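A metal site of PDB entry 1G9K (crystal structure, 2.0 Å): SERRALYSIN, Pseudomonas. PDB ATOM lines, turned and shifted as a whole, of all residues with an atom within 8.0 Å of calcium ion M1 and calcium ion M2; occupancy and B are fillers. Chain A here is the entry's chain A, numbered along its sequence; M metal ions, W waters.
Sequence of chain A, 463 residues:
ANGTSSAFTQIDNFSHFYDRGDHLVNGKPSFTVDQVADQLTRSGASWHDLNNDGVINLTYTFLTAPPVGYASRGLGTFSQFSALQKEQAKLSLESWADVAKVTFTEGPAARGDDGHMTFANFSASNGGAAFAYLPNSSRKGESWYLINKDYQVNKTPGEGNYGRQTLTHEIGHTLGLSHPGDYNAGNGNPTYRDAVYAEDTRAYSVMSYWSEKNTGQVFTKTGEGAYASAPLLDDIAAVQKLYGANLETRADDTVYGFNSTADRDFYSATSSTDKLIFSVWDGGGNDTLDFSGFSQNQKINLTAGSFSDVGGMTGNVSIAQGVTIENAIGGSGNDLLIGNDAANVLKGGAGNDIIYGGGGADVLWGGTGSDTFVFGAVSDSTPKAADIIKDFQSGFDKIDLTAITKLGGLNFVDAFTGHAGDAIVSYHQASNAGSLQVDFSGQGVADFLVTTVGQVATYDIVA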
ATOM      1  N   GLU A 248      14.798   7.735  15.586  1.00  0.00           N
ATOM      2  CA  GLU A 248      14.060   8.230  16.744  1.00  0.00           C
ATOM      3  C   GLU A 248      13.527   7.094  17.614  1.00  0.00           C
ATOM      4  O   GLU A 248      13.272   7.272  18.806  1.00  0.00           O
ATOM      5  CB  GLU A 248      12.888   9.066  16.261  1.00  0.00           C
ATOM      6  CG  GLU A 248      13.247  10.102  15.210  1.00  0.00           C
ATOM      7  CD  GLU A 248      13.511  11.472  15.797  1.00  0.00           C
ATOM      8  OE1 GLU A 248      14.455  11.602  16.608  1.00  0.00           O
ATOM      9  OE2 GLU A 248      12.758  12.400  15.457  1.00  0.00           O
ATOM     10  N   THR A 249      13.383   5.918  17.014  1.00  0.00           N
ATOM     11  CA  THR A 249      12.835   4.761  17.691  1.00  0.00           C
ATOM     12  C   THR A 249      13.688   4.140  18.804  1.00  0.00           C
ATOM     13  O   THR A 249      14.836   3.755  18.582  1.00  0.00           O
ATOM     14  CB  THR A 249      12.503   3.659  16.666  1.00  0.00           C
ATOM     15  OG1 THR A 249      11.646   4.213  15.663  1.00  0.00           O
ATOM     16  CG2 THR A 249      11.794   2.498  17.333  1.00  0.00           C
ATOM     17  N   ARG A 250      13.097   4.035  19.999  1.00  0.00           N
ATOM     18  CA  ARG A 250      13.784   3.462  21.145  1.00  0.00           C
ATOM     19  C   ARG A 250      15.197   4.049  21.275  1.00  0.00           C
ATOM     20  O   ARG A 250      16.155   3.323  21.516  1.00  0.00           O
ATOM     21  CB  ARG A 250      13.824   1.932  20.987  1.00  0.00           C
ATOM     22  CG  ARG A 250      12.414   1.273  20.972  1.00  0.00           C
ATOM     23  CD  ARG A 250      12.469  -0.251  20.849  1.00  0.00           C
ATOM     24  NE  ARG A 250      12.786  -0.701  19.503  1.00  0.00           N
ATOM     25  CZ  ARG A 250      11.911  -0.829  18.509  1.00  0.00           C
ATOM     26  NH1 ARG A 250      10.634  -0.534  18.709  1.00  0.00           N
ATOM     27  NH2 ARG A 250      12.307  -1.245  17.309  1.00  0.00           N
ATOM     28  N   ALA A 251      15.315   5.362  21.115  1.00  0.00           N
ATOM     29  CA  ALA A 251      16.599   6.045  21.184  1.00  0.00           C
ATOM     30  C   ALA A 251      17.219   6.132  22.588  1.00  0.00           C
ATOM     31  O   ALA A 251      18.342   6.596  22.737  1.00  0.00           O
ATOM     32  CB  ALA A 251      16.473   7.451  20.590  1.00  0.00           C
ATOM     33  N   ASP A 252      16.481   5.677  23.601  1.00  0.00           N
ATOM     34  CA  ASP A 252      16.966   5.680  24.979  1.00  0.00           C
ATOM     35  C   ASP A 252      17.348   4.247  25.355  1.00  0.00           C
ATOM     36  O   ASP A 252      17.270   3.348  24.529  1.00  0.00           O
ATOM     37  CB  ASP A 252      15.889   6.204  25.926  1.00  0.00           C
ATOM     38  CG  ASP A 252      14.568   5.473  25.768  1.00  0.00           C
ATOM     39  OD1 ASP A 252      13.682   5.648  26.631  1.00  0.00           O
ATOM     40  OD2 ASP A 252      14.406   4.722  24.781  1.00  0.00           O
ATOM     41  N   ASP A 253      17.776   4.036  26.607  1.00  0.00           N
ATOM     42  CA  ASP A 253      18.156   2.702  27.064  1.00  0.00           C
ATOM     43  C   ASP A 253      16.998   1.730  26.890  1.00  0.00           C
ATOM     44  O   ASP A 253      15.893   1.972  27.385  1.00  0.00           O
ATOM     45  CB  ASP A 253      18.580   2.744  28.541  1.00  0.00           C
ATOM     46  CG  ASP A 253      19.825   3.572  28.788  1.00  0.00           C
ATOM     47  OD1 ASP A 253      20.375   4.129  27.804  1.00  0.00           O
ATOM     48  OD2 ASP A 253      20.254   3.670  29.955  1.00  0.00           O
ATOM     49  N   THR A 254      17.250   0.629  26.188  1.00  0.00           N
ATOM     50  CA  THR A 254      16.187  -0.346  25.920  1.00  0.00           C
ATOM     51  C   THR A 254      16.565  -1.776  26.263  1.00  0.00           C
ATOM     52  O   THR A 254      17.697  -2.195  26.056  1.00  0.00           O
ATOM     53  CB  THR A 254      15.788  -0.310  24.436  1.00  0.00           C
ATOM     54  OG1 THR A 254      15.796   1.048  23.973  1.00  0.00           O
ATOM     55  CG2 THR A 254      14.392  -0.886  24.252  1.00  0.00           C
ATOM     56  N   VAL A 255      15.599  -2.534  26.777  1.00  0.00           N
ATOM     57  CA  VAL A 255      15.819  -3.928  27.096  1.00  0.00           C
ATOM     58  C   VAL A 255      14.895  -4.764  26.204  1.00  0.00           C
ATOM     59  O   VAL A 255      13.711  -4.458  26.083  1.00  0.00           O
ATOM     60  CB  VAL A 255      15.508  -4.245  28.584  1.00  0.00           C
ATOM     61  CG1 VAL A 255      15.788  -5.716  28.864  1.00  0.00           C
ATOM     62  CG2 VAL A 255      16.353  -3.363  29.496  1.00  0.00           C
ATOM     63  N   TYR A 256      15.451  -5.787  25.559  1.00  0.00           N
ATOM     64  CA  TYR A 256      14.690  -6.685  24.686  1.00  0.00           C
ATOM     65  C   TYR A 256      14.715  -8.085  25.294  1.00  0.00           C
ATOM     66  O   TYR A 256      15.695  -8.464  25.930  1.00  0.00           O
ATOM     67  CB  TYR A 256      15.308  -6.744  23.279  1.00  0.00           C
ATOM     68  CG  TYR A 256      15.364  -5.415  22.566  1.00  0.00           C
ATOM     69  CD1 TYR A 256      16.385  -4.499  22.828  1.00  0.00           C
ATOM     70  CD2 TYR A 256      14.359  -5.051  21.668  1.00  0.00           C
ATOM     71  CE1 TYR A 256      16.399  -3.236  22.213  1.00  0.00           C
ATOM     72  CE2 TYR A 256      14.366  -3.811  21.051  1.00  0.00           C
ATOM     73  CZ  TYR A 256      15.378  -2.906  21.331  1.00  0.00           C
ATOM     74  OH  TYR A 256      15.350  -1.669  20.736  1.00  0.00           O
ATOM     75  N   THR A 261      11.563  -3.585  27.707  1.00  0.00           N
ATOM     76  CA  THR A 261      11.062  -2.223  27.848  1.00  0.00           C
ATOM     77  C   THR A 261      10.832  -1.645  26.456  1.00  0.00           C
ATOM     78  O   THR A 261      10.645  -0.439  26.289  1.00  0.00           O
ATOM     79  CB  THR A 261      12.048  -1.312  28.605  1.00  0.00           C
ATOM     80  OG1 THR A 261      13.300  -1.263  27.905  1.00  0.00           O
ATOM     81  CG2 THR A 261      12.288  -1.838  30.012  1.00  0.00           C
ATOM     82  N   VAL A 280      16.463  -6.927  15.803  1.00  0.00           N
ATOM     83  CA  VAL A 280      16.502  -5.721  16.619  1.00  0.00           C
ATOM     84  C   VAL A 280      16.826  -4.426  15.868  1.00  0.00           C
ATOM     85  O   VAL A 280      17.839  -4.334  15.180  1.00  0.00           O
ATOM     86  CB  VAL A 280      17.535  -5.887  17.774  1.00  0.00           C
ATOM     87  CG1 VAL A 280      17.577  -4.620  18.631  1.00  0.00           C
ATOM     88  CG2 VAL A 280      17.175  -7.086  18.627  1.00  0.00           C
ATOM     89  N   TRP A 281      15.940  -3.440  15.984  1.00  0.00           N
ATOM     90  CA  TRP A 281      16.191  -2.131  15.402  1.00  0.00           C
ATOM     91  C   TRP A 281      16.107  -1.206  16.609  1.00  0.00           C
ATOM     92  O   TRP A 281      15.147  -1.259  17.370  1.00  0.00           O
ATOM     93  CB  TRP A 281      15.161  -1.724  14.354  1.00  0.00           C
ATOM     94  CG  TRP A 281      15.312  -0.266  13.976  1.00  0.00           C
ATOM     95  CD1 TRP A 281      14.470   0.764  14.324  1.00  0.00           C
ATOM     96  CD2 TRP A 281      16.446   0.346  13.349  1.00  0.00           C
ATOM     97  NE1 TRP A 281      15.020   1.963  13.956  1.00  0.00           N
ATOM     98  CE2 TRP A 281      16.226   1.741  13.351  1.00  0.00           C
ATOM     99  CE3 TRP A 281      17.638  -0.153  12.782  1.00  0.00           C
ATOM    100  CZ2 TRP A 281      17.153   2.647  12.817  1.00  0.00           C
ATOM    101  CZ3 TRP A 281      18.555   0.752  12.236  1.00  0.00           C
ATOM    102  CH2 TRP A 281      18.306   2.138  12.265  1.00  0.00           C
ATOM    103  N   ASP A 282      17.126  -0.366  16.781  1.00  0.00           N
ATOM    104  CA  ASP A 282      17.200   0.552  17.913  1.00  0.00           C
ATOM    105  C   ASP A 282      17.934   1.831  17.500  1.00  0.00           C
ATOM    106  O   ASP A 282      18.945   1.777  16.803  1.00  0.00           O
ATOM    107  CB  ASP A 282      17.951  -0.166  19.048  1.00  0.00           C
ATOM    108  CG  ASP A 282      17.917   0.603  20.360  1.00  0.00           C
ATOM    109  OD1 ASP A 282      18.573   1.661  20.455  1.00  0.00           O
ATOM    110  OD2 ASP A 282      17.222   0.140  21.279  1.00  0.00           O
ATOM    111  N   GLY A 283      17.410   2.977  17.920  1.00  0.00           N
ATOM    112  CA  GLY A 283      17.997   4.250  17.543  1.00  0.00           C
ATOM    113  C   GLY A 283      19.185   4.773  18.351  1.00  0.00           C
ATOM    114  O   GLY A 283      19.926   5.633  17.871  1.00  0.00           O
ATOM    115  N   GLY A 284      19.355   4.265  19.564  1.00  0.00           N
ATOM    116  CA  GLY A 284      20.472   4.729  20.381  1.00  0.00           C
ATOM    117  C   GLY A 284      20.306   4.379  21.847  1.00  0.00           C
ATOM    118  O   GLY A 284      19.300   3.775  22.236  1.00  0.00           O
ATOM    119  N   GLY A 285      21.290   4.758  22.655  1.00  0.00           N
ATOM    120  CA  GLY A 285      21.239   4.489  24.079  1.00  0.00           C
ATOM    121  C   GLY A 285      22.011   3.250  24.496  1.00  0.00           C
ATOM    122  O   GLY A 285      22.658   2.605  23.673  1.00  0.00           O
ATOM    123  N   ASN A 286      21.950   2.924  25.781  1.00  0.00           N
ATOM    124  CA  ASN A 286      22.636   1.752  26.327  1.00  0.00           C
ATOM    125  C   ASN A 286      21.578   0.648  26.384  1.00  0.00           C
ATOM    126  O   ASN A 286      20.689   0.677  27.238  1.00  0.00           O
ATOM    127  CB  ASN A 286      23.175   2.033  27.726  1.00  0.00           C
ATOM    128  CG  ASN A 286      24.020   0.896  28.261  1.00  0.00           C
ATOM    129  OD1 ASN A 286      25.147   0.683  27.802  1.00  0.00           O
ATOM    130  ND2 ASN A 286      23.486   0.164  29.213  1.00  0.00           N
ATOM    131  N   ASP A 287      21.714  -0.322  25.494  1.00  0.00           N
ATOM    132  CA  ASP A 287      20.743  -1.404  25.349  1.00  0.00           C
ATOM    133  C   ASP A 287      21.195  -2.797  25.756  1.00  0.00           C
ATOM    134  O   ASP A 287      22.370  -3.134  25.658  1.00  0.00           O
ATOM    135  CB  ASP A 287      20.276  -1.408  23.899  1.00  0.00           C
ATOM    136  CG  ASP A 287      20.085  -0.012  23.383  1.00  0.00           C
ATOM    137  OD1 ASP A 287      19.196   0.688  23.897  1.00  0.00           O
ATOM    138  OD2 ASP A 287      20.838   0.398  22.462  1.00  0.00           O
ATOM    139  N   THR A 288      20.231  -3.624  26.187  1.00  0.00           N
ATOM    140  CA  THR A 288      20.538  -4.972  26.634  1.00  0.00           C
ATOM    141  C   THR A 288      19.618  -6.052  26.056  1.00  0.00           C
ATOM    142  O   THR A 288      18.420  -5.838  25.886  1.00  0.00           O
ATOM    143  CB  THR A 288      20.469  -5.048  28.168  1.00  0.00           C
ATOM    144  OG1 THR A 288      21.168  -3.925  28.733  1.00  0.00           O
ATOM    145  CG2 THR A 288      21.103  -6.334  28.662  1.00  0.00           C
ATOM    146  N   VAL A 323      23.128  -0.913  13.900  1.00  0.00           N
ATOM    147  CA  VAL A 323      22.662  -0.864  15.287  1.00  0.00           C
ATOM    148  C   VAL A 323      23.720  -1.378  16.251  1.00  0.00           C
ATOM    149  O   VAL A 323      24.341  -2.404  16.013  1.00  0.00           O
ATOM    150  CB  VAL A 323      21.370  -1.697  15.461  1.00  0.00           C
ATOM    151  CG1 VAL A 323      20.950  -1.706  16.924  1.00  0.00           C
ATOM    152  CG2 VAL A 323      20.261  -1.133  14.596  1.00  0.00           C
ATOM    153  N   THR A 324      23.926  -0.639  17.342  1.00  0.00           N
ATOM    154  CA  THR A 324      24.895  -1.054  18.351  1.00  0.00           C
ATOM    155  C   THR A 324      24.190  -1.408  19.652  1.00  0.00           C
ATOM    156  O   THR A 324      23.610  -0.538  20.307  1.00  0.00           O
ATOM    157  CB  THR A 324      25.944   0.052  18.652  1.00  0.00           C
ATOM    158  OG1 THR A 324      26.605   0.437  17.437  1.00  0.00           O
ATOM    159  CG2 THR A 324      26.978  -0.456  19.638  1.00  0.00           C
ATOM    160  N   ILE A 325      24.212  -2.689  20.008  1.00  0.00           N
ATOM    161  CA  ILE A 325      23.608  -3.188  21.246  1.00  0.00           C
ATOM    162  C   ILE A 325      24.780  -3.407  22.196  1.00  0.00           C
ATOM    163  O   ILE A 325      25.730  -4.126  21.865  1.00  0.00           O
ATOM    164  CB  ILE A 325      22.865  -4.511  21.035  1.00  0.00           C
ATOM    165  CG1 ILE A 325      21.797  -4.347  19.948  1.00  0.00           C
ATOM    166  CG2 ILE A 325      22.225  -4.978  22.350  1.00  0.00           C
ATOM    167  CD1 ILE A 325      20.769  -3.271  20.262  1.00  0.00           C
ATOM    168  N   GLU A 326      24.683  -2.816  23.375  1.00  0.00           N
ATOM    169  CA  GLU A 326      25.748  -2.875  24.373  1.00  0.00           C
ATOM    170  C   GLU A 326      25.850  -4.075  25.307  1.00  0.00           C
ATOM    171  O   GLU A 326      26.953  -4.570  25.577  1.00  0.00           O
ATOM    172  CB  GLU A 326      25.695  -1.609  25.248  1.00  0.00           C
ATOM    173  CG  GLU A 326      25.985  -0.296  24.527  1.00  0.00           C
ATOM    174  CD  GLU A 326      24.932   0.096  23.509  1.00  0.00           C
ATOM    175  OE1 GLU A 326      23.747  -0.268  23.664  1.00  0.00           O
ATOM    176  OE2 GLU A 326      25.292   0.787  22.533  1.00  0.00           O
ATOM    177  N   ASN A 327      24.712  -4.541  25.815  1.00  0.00           N
ATOM    178  CA  ASN A 327      24.724  -5.640  26.777  1.00  0.00           C
ATOM    179  C   ASN A 327      23.903  -6.873  26.422  1.00  0.00           C
ATOM    180  O   ASN A 327      22.965  -6.809  25.642  1.00  0.00           O
ATOM    181  CB  ASN A 327      24.258  -5.120  28.137  1.00  0.00           C
ATOM    182  CG  ASN A 327      24.739  -3.716  28.424  1.00  0.00           C
ATOM    183  OD1 ASN A 327      25.938  -3.428  28.318  1.00  0.00           O
ATOM    184  ND2 ASN A 327      23.819  -2.830  28.803  1.00  0.00           N
ATOM    185  N   ASN A 340      30.959  -6.756  21.145  1.00  0.00           N
ATOM    186  CA  ASN A 340      31.420  -6.025  19.973  1.00  0.00           C
ATOM    187  C   ASN A 340      32.513  -5.025  20.375  1.00  0.00           C
ATOM    188  O   ASN A 340      33.045  -5.094  21.488  1.00  0.00           O
ATOM    189  CB  ASN A 340      30.249  -5.290  19.316  1.00  0.00           C
ATOM    190  CG  ASN A 340      29.370  -4.563  20.311  1.00  0.00           C
ATOM    191  OD1 ASN A 340      29.861  -3.902  21.229  1.00  0.00           O
ATOM    192  ND2 ASN A 340      28.053  -4.679  20.135  1.00  0.00           N
ATOM    193  N   ALA A 342      32.274  -2.054  21.233  1.00  0.00           N
ATOM    194  CA  ALA A 342      31.883  -1.146  22.295  1.00  0.00           C
ATOM    195  C   ALA A 342      32.082  -1.784  23.661  1.00  0.00           C
ATOM    196  O   ALA A 342      32.333  -2.990  23.762  1.00  0.00           O
ATOM    197  CB  ALA A 342      30.432  -0.727  22.104  1.00  0.00           C
HETATM  198 CA    CA M   1      22.914   1.162  21.795  1.00  0.00          CA
HETATM  199 CA    CA M   2      17.716   2.015  22.732  1.00  0.00          CA
HETATM  200  O   HOH W   1      24.095   3.147  20.537  1.00  0.00           O
HETATM  201  O   HOH W   2      21.338   1.605  20.036  1.00  0.00           O
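Calcium ion M2 is bound by O of Asp 252 (2.3 Å), OD1 of Asp 287 (2.3 Å), O of Arg 250 (2.4 Å), O of Gly 284 (2.4 Å), OD2 of Asp 282 (2.4 Å), OD1 of Asp 282 (2.5 Å) and OG1 of Thr 254 (2.5 Å).
Calcium ion M2 has seven donor atoms within binding distance.
The backbone carbonyl oxygen (O) of Asp 287 sits at hydrogen-bond distance from the backbone NH (N) of Asn 327 (2.7 Å).
OH of Tyr 256 lies within hydrogen-bond range of NE of Arg 250 (3.0 Å).
The backbone carbonyl oxygen (O) of Trp 281 sits at hydrogen-bond distance from the guanidinium group (NH2) of Arg 250, 2.8 Å away.
The backbone NH (N) of Gly 285 sits at hydrogen-bond distance from the backbone carbonyl oxygen (O) of Ala 251, at 3.5 Å.
The side-chain hydroxyl (OH) of Tyr 256 lies close to the side-chain carboxylate (OD2) of Asp 282 (2.7 Å).
The backbone carbonyl oxygen of Thr 254 is in hydrogen-bond range of the backbone NH of Thr 288, at 2.9 Å.
Within 4 Å of calcium ion M1: Gly 285, Asp 287, Thr 324 and Glu 326.
The nearest printed residue that does not touch calcium ion M1 is Gly 284 (4.1 Å).
Within 4 Å of calcium ion M2: Arg 250, Asp 252, Thr 254, Asp 282, Gly 284 and Asp 287.
Along chain A the residues within 4 Å of calcium ion M2 span positions 250 to 287.
The nearest printed residue that does not touch calcium ion M2 is Ala 251 (4.1 Å).
Calcium ion M1 is bound by OD2 of Asp 287 (2.3 Å), O of Thr 324 (2.4 Å), O of Gly 285 (2.4 Å), water W2 (2.4 Å), OE1 of Glu 326 (2.5 Å), OE2 of Glu 326 (2.5 Å) and water W1 (2.6 Å).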
